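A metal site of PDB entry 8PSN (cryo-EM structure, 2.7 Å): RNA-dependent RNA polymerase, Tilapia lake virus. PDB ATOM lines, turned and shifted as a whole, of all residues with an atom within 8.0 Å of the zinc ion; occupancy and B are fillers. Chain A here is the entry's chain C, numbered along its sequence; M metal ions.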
ATOM      1  N   THR A 145      -9.122  24.586  19.241  1.00  0.00           N
ATOM      2  CA  THR A 145      -8.150  25.052  20.219  1.00  0.00           C
ATOM      3  C   THR A 145      -6.740  24.535  19.915  1.00  0.00           C
ATOM      4  O   THR A 145      -5.766  25.225  20.213  1.00  0.00           O
ATOM      5  CB  THR A 145      -8.565  24.638  21.623  1.00  0.00           C
ATOM      6  OG1 THR A 145      -8.936  23.245  21.626  1.00  0.00           O
ATOM      7  CG2 THR A 145      -9.754  25.470  22.091  1.00  0.00           C
ATOM      8  N   CYS A 146      -6.634  23.340  19.341  1.00  0.00           N
ATOM      9  CA  CYS A 146      -5.314  22.769  19.103  1.00  0.00           C
ATOM     10  C   CYS A 146      -4.525  23.585  18.094  1.00  0.00           C
ATOM     11  O   CYS A 146      -3.322  23.770  18.238  1.00  0.00           O
ATOM     12  CB  CYS A 146      -5.440  21.313  18.642  1.00  0.00           C
ATOM     13  SG  CYS A 146      -5.360  20.126  19.999  1.00  0.00           S
ATOM     14  N   GLU A 147      -5.190  24.076  17.039  1.00  0.00           N
ATOM     15  CA  GLU A 147      -4.517  24.955  16.085  1.00  0.00           C
ATOM     16  C   GLU A 147      -3.986  26.198  16.774  1.00  0.00           C
ATOM     17  O   GLU A 147      -2.834  26.603  16.552  1.00  0.00           O
ATOM     18  CB  GLU A 147      -5.474  25.341  14.966  1.00  0.00           C
ATOM     19  CG  GLU A 147      -4.787  25.844  13.724  1.00  0.00           C
ATOM     20  CD  GLU A 147      -5.561  25.525  12.460  1.00  0.00           C
ATOM     21  OE1 GLU A 147      -5.042  24.766  11.630  1.00  0.00           O
ATOM     22  OE2 GLU A 147      -6.692  26.023  12.312  1.00  0.00           O
ATOM     23  N   SER A 148      -4.799  26.831  17.620  1.00  0.00           N
ATOM     24  CA  SER A 148      -4.359  28.038  18.306  1.00  0.00           C
ATOM     25  C   SER A 148      -3.197  27.751  19.242  1.00  0.00           C
ATOM     26  O   SER A 148      -2.267  28.559  19.363  1.00  0.00           O
ATOM     27  CB  SER A 148      -5.528  28.659  19.074  1.00  0.00           C
ATOM     28  OG  SER A 148      -6.739  28.480  18.379  1.00  0.00           O
ATOM     29  N   GLY A 149      -3.229  26.602  19.919  1.00  0.00           N
ATOM     30  CA  GLY A 149      -2.168  26.264  20.848  1.00  0.00           C
ATOM     31  C   GLY A 149      -0.869  25.847  20.179  1.00  0.00           C
ATOM     32  O   GLY A 149       0.210  26.056  20.736  1.00  0.00           O
ATOM     33  N   PHE A 150      -0.952  25.264  18.987  1.00  0.00           N
ATOM     34  CA  PHE A 150       0.253  24.831  18.303  1.00  0.00           C
ATOM     35  C   PHE A 150       1.165  26.010  17.976  1.00  0.00           C
ATOM     36  O   PHE A 150       2.382  25.944  18.169  1.00  0.00           O
ATOM     37  CB  PHE A 150      -0.106  24.073  17.019  1.00  0.00           C
ATOM     38  CG  PHE A 150       1.080  23.514  16.288  1.00  0.00           C
ATOM     39  CD1 PHE A 150       1.906  22.583  16.889  1.00  0.00           C
ATOM     40  CD2 PHE A 150       1.372  23.936  15.006  1.00  0.00           C
ATOM     41  CE1 PHE A 150       3.005  22.077  16.215  1.00  0.00           C
ATOM     42  CE2 PHE A 150       2.467  23.439  14.332  1.00  0.00           C
ATOM     43  CZ  PHE A 150       3.285  22.505  14.936  1.00  0.00           C
ATOM     44  N   PRO A 155       0.766  27.848  25.208  1.00  0.00           N
ATOM     45  CA  PRO A 155      -0.671  27.582  25.070  1.00  0.00           C
ATOM     46  C   PRO A 155      -1.399  27.742  26.399  1.00  0.00           C
ATOM     47  O   PRO A 155      -0.874  27.410  27.458  1.00  0.00           O
ATOM     48  CB  PRO A 155      -0.725  26.132  24.569  1.00  0.00           C
ATOM     49  CG  PRO A 155       0.646  25.853  24.023  1.00  0.00           C
ATOM     50  CD  PRO A 155       1.579  26.666  24.847  1.00  0.00           C
ATOM     51  N   THR A 157      -4.403  26.280  27.333  1.00  0.00           N
ATOM     52  CA  THR A 157      -5.013  25.040  27.814  1.00  0.00           C
ATOM     53  C   THR A 157      -4.299  23.836  27.213  1.00  0.00           C
ATOM     54  O   THR A 157      -4.558  23.475  26.051  1.00  0.00           O
ATOM     55  CB  THR A 157      -6.499  24.998  27.473  1.00  0.00           C
ATOM     56  OG1 THR A 157      -6.669  25.042  26.054  1.00  0.00           O
ATOM     57  CG2 THR A 157      -7.229  26.164  28.108  1.00  0.00           C
ATOM     58  N   PRO A 158      -3.391  23.176  27.942  1.00  0.00           N
ATOM     59  CA  PRO A 158      -2.781  21.954  27.406  1.00  0.00           C
ATOM     60  C   PRO A 158      -3.816  20.857  27.246  1.00  0.00           C
ATOM     61  O   PRO A 158      -4.791  20.768  27.996  1.00  0.00           O
ATOM     62  CB  PRO A 158      -1.742  21.589  28.468  1.00  0.00           C
ATOM     63  CG  PRO A 158      -2.174  22.271  29.712  1.00  0.00           C
ATOM     64  CD  PRO A 158      -2.865  23.528  29.275  1.00  0.00           C
ATOM     65  N   CYS A 159      -3.596  20.010  26.242  1.00  0.00           N
ATOM     66  CA  CYS A 159      -4.488  18.890  25.943  1.00  0.00           C
ATOM     67  C   CYS A 159      -3.815  17.536  26.155  1.00  0.00           C
ATOM     68  O   CYS A 159      -4.404  16.503  25.800  1.00  0.00           O
ATOM     69  CB  CYS A 159      -5.002  18.992  24.507  1.00  0.00           C
ATOM     70  SG  CYS A 159      -3.719  18.891  23.247  1.00  0.00           S
ATOM     71  N   GLY A 160      -2.617  17.502  26.719  1.00  0.00           N
ATOM     72  CA  GLY A 160      -1.918  16.244  26.914  1.00  0.00           C
ATOM     73  C   GLY A 160      -1.243  15.700  25.683  1.00  0.00           C
ATOM     74  O   GLY A 160      -0.903  14.512  25.658  1.00  0.00           O
ATOM     75  N   PHE A 161      -1.034  16.524  24.658  1.00  0.00           N
ATOM     76  CA  PHE A 161      -0.395  16.106  23.429  1.00  0.00           C
ATOM     77  C   PHE A 161       0.669  17.128  23.049  1.00  0.00           C
ATOM     78  O   PHE A 161       0.707  18.250  23.569  1.00  0.00           O
ATOM     79  CB  PHE A 161      -1.409  15.932  22.299  1.00  0.00           C
ATOM     80  CG  PHE A 161      -2.236  14.674  22.411  1.00  0.00           C
ATOM     81  CD1 PHE A 161      -1.769  13.483  21.892  1.00  0.00           C
ATOM     82  CD2 PHE A 161      -3.460  14.701  23.042  1.00  0.00           C
ATOM     83  CE1 PHE A 161      -2.522  12.330  22.001  1.00  0.00           C
ATOM     84  CE2 PHE A 161      -4.222  13.544  23.155  1.00  0.00           C
ATOM     85  CZ  PHE A 161      -3.750  12.365  22.632  1.00  0.00           C
ATOM     86  N   ILE A 162       1.536  16.730  22.109  1.00  0.00           N
ATOM     87  CA  ILE A 162       2.721  17.532  21.785  1.00  0.00           C
ATOM     88  C   ILE A 162       2.336  18.907  21.252  1.00  0.00           C
ATOM     89  O   ILE A 162       3.113  19.859  21.386  1.00  0.00           O
ATOM     90  CB  ILE A 162       3.624  16.771  20.796  1.00  0.00           C
ATOM     91  CG1 ILE A 162       5.087  17.167  20.999  1.00  0.00           C
ATOM     92  CG2 ILE A 162       3.186  17.043  19.366  1.00  0.00           C
ATOM     93  CD1 ILE A 162       6.069  16.114  20.529  1.00  0.00           C
ATOM     94  N   CYS A 163       1.162  19.025  20.632  1.00  0.00           N
ATOM     95  CA  CYS A 163       0.799  20.299  20.011  1.00  0.00           C
ATOM     96  C   CYS A 163       0.688  21.415  21.045  1.00  0.00           C
ATOM     97  O   CYS A 163       1.207  22.517  20.840  1.00  0.00           O
ATOM     98  CB  CYS A 163      -0.516  20.153  19.241  1.00  0.00           C
ATOM     99  SG  CYS A 163      -1.736  19.078  20.027  1.00  0.00           S
ATOM    100  N   CYS A 164       0.023  21.144  22.174  1.00  0.00           N
ATOM    101  CA  CYS A 164      -0.263  22.159  23.174  1.00  0.00           C
ATOM    102  C   CYS A 164       0.467  21.924  24.485  1.00  0.00           C
ATOM    103  O   CYS A 164       0.122  22.561  25.497  1.00  0.00           O
ATOM    104  CB  CYS A 164      -1.774  22.237  23.419  1.00  0.00           C
ATOM    105  SG  CYS A 164      -2.758  22.249  21.897  1.00  0.00           S
ATOM    106  N   GLY A 165       1.457  21.045  24.514  1.00  0.00           N
ATOM    107  CA  GLY A 165       2.195  20.747  25.713  1.00  0.00           C
ATOM    108  C   GLY A 165       2.964  19.456  25.573  1.00  0.00           C
ATOM    109  O   GLY A 165       2.986  18.841  24.509  1.00  0.00           O
ATOM    110  N   SER A 168       2.260  13.074  23.359  1.00  0.00           N
ATOM    111  CA  SER A 168       2.448  12.307  22.148  1.00  0.00           C
ATOM    112  C   SER A 168       1.755  13.000  20.972  1.00  0.00           C
ATOM    113  O   SER A 168       1.250  14.126  21.093  1.00  0.00           O
ATOM    114  CB  SER A 168       1.942  10.877  22.362  1.00  0.00           C
ATOM    115  OG  SER A 168       0.822  10.863  23.242  1.00  0.00           O
ATOM    116  N   LYS A 170      -1.031  13.630  18.021  1.00  0.00           N
ATOM    117  CA  LYS A 170      -2.425  13.461  17.622  1.00  0.00           C
ATOM    118  C   LYS A 170      -2.491  13.029  16.158  1.00  0.00           C
ATOM    119  O   LYS A 170      -1.480  12.918  15.472  1.00  0.00           O
ATOM    120  CB  LYS A 170      -3.197  14.774  17.825  1.00  0.00           C
ATOM    121  CG  LYS A 170      -3.891  14.894  19.169  1.00  0.00           C
ATOM    122  CD  LYS A 170      -4.433  16.297  19.365  1.00  0.00           C
ATOM    123  CE  LYS A 170      -5.009  16.475  20.762  1.00  0.00           C
ATOM    124  NZ  LYS A 170      -6.201  17.372  20.764  1.00  0.00           N
ATOM    125  N   LEU A 173      -1.343  15.790  13.481  1.00  0.00           N
ATOM    126  CA  LEU A 173       0.056  16.200  13.478  1.00  0.00           C
ATOM    127  C   LEU A 173       0.895  15.202  12.685  1.00  0.00           C
ATOM    128  O   LEU A 173       0.475  14.076  12.422  1.00  0.00           O
ATOM    129  CB  LEU A 173       0.597  16.302  14.913  1.00  0.00           C
ATOM    130  CG  LEU A 173      -0.129  17.271  15.852  1.00  0.00           C
ATOM    131  CD1 LEU A 173       0.336  17.064  17.271  1.00  0.00           C
ATOM    132  CD2 LEU A 173       0.088  18.702  15.414  1.00  0.00           C
ATOM    133  N   ARG A 245       7.576  19.892  25.063  1.00  0.00           N
ATOM    134  CA  ARG A 245       7.224  20.960  24.136  1.00  0.00           C
ATOM    135  C   ARG A 245       7.935  22.236  24.554  1.00  0.00           C
ATOM    136  O   ARG A 245       7.744  22.721  25.673  1.00  0.00           O
ATOM    137  CB  ARG A 245       5.717  21.173  24.095  1.00  0.00           C
ATOM    138  CG  ARG A 245       5.223  21.922  22.865  1.00  0.00           C
ATOM    139  CD  ARG A 245       4.648  23.282  23.212  1.00  0.00           C
ATOM    140  NE  ARG A 245       3.661  23.724  22.225  1.00  0.00           N
ATOM    141  CZ  ARG A 245       3.391  24.987  21.928  1.00  0.00           C
ATOM    142  NH1 ARG A 245       4.024  25.978  22.523  1.00  0.00           N
ATOM    143  NH2 ARG A 245       2.477  25.254  21.008  1.00  0.00           N
ATOM    144  N   HIS A 266       1.861  20.687  11.684  1.00  0.00           N
ATOM    145  CA  HIS A 266       0.404  20.579  11.766  1.00  0.00           C
ATOM    146  C   HIS A 266      -0.179  20.654  10.361  1.00  0.00           C
ATOM    147  O   HIS A 266       0.257  21.464   9.543  1.00  0.00           O
ATOM    148  CB  HIS A 266      -0.180  21.689  12.648  1.00  0.00           C
ATOM    149  CG  HIS A 266      -1.573  21.399  13.127  1.00  0.00           C
ATOM    150  ND1 HIS A 266      -2.676  21.540  12.324  1.00  0.00           N
ATOM    151  CD2 HIS A 266      -2.024  20.999  14.336  1.00  0.00           C
ATOM    152  CE1 HIS A 266      -3.756  21.227  13.012  1.00  0.00           C
ATOM    153  NE2 HIS A 266      -3.394  20.899  14.231  1.00  0.00           N
HETATM  154 ZN    ZN M   1      -3.410  20.100  21.280  1.00  0.00          ZN
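NZ of Lys 170 touches the zinc ion, at 3.9 Å.
Of the 21 residues printed, 5 come within 4 Å of the zinc ion.
The nearest printed residue that does not touch the zinc ion is Phe 161 (4.7 Å).
The zinc ion is bound by the side-chain sulfur (SG) of Cys 163 (2.3 Å), the side-chain sulfur (SG) of Cys 164 (2.3 Å), the side-chain sulfur (SG) of Cys 159 (2.3 Å) and the side-chain sulfur (SG) of Cys 146 (2.3 Å).
The zinc ion has four donor atoms within binding distance.
O of Cys 163 sits at hydrogen-bond distance from NH2 of Arg 245.
The side-chain sulfur of Cys 146 sits close to the side-chain amino group of Lys 170, at 3.0 Å.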
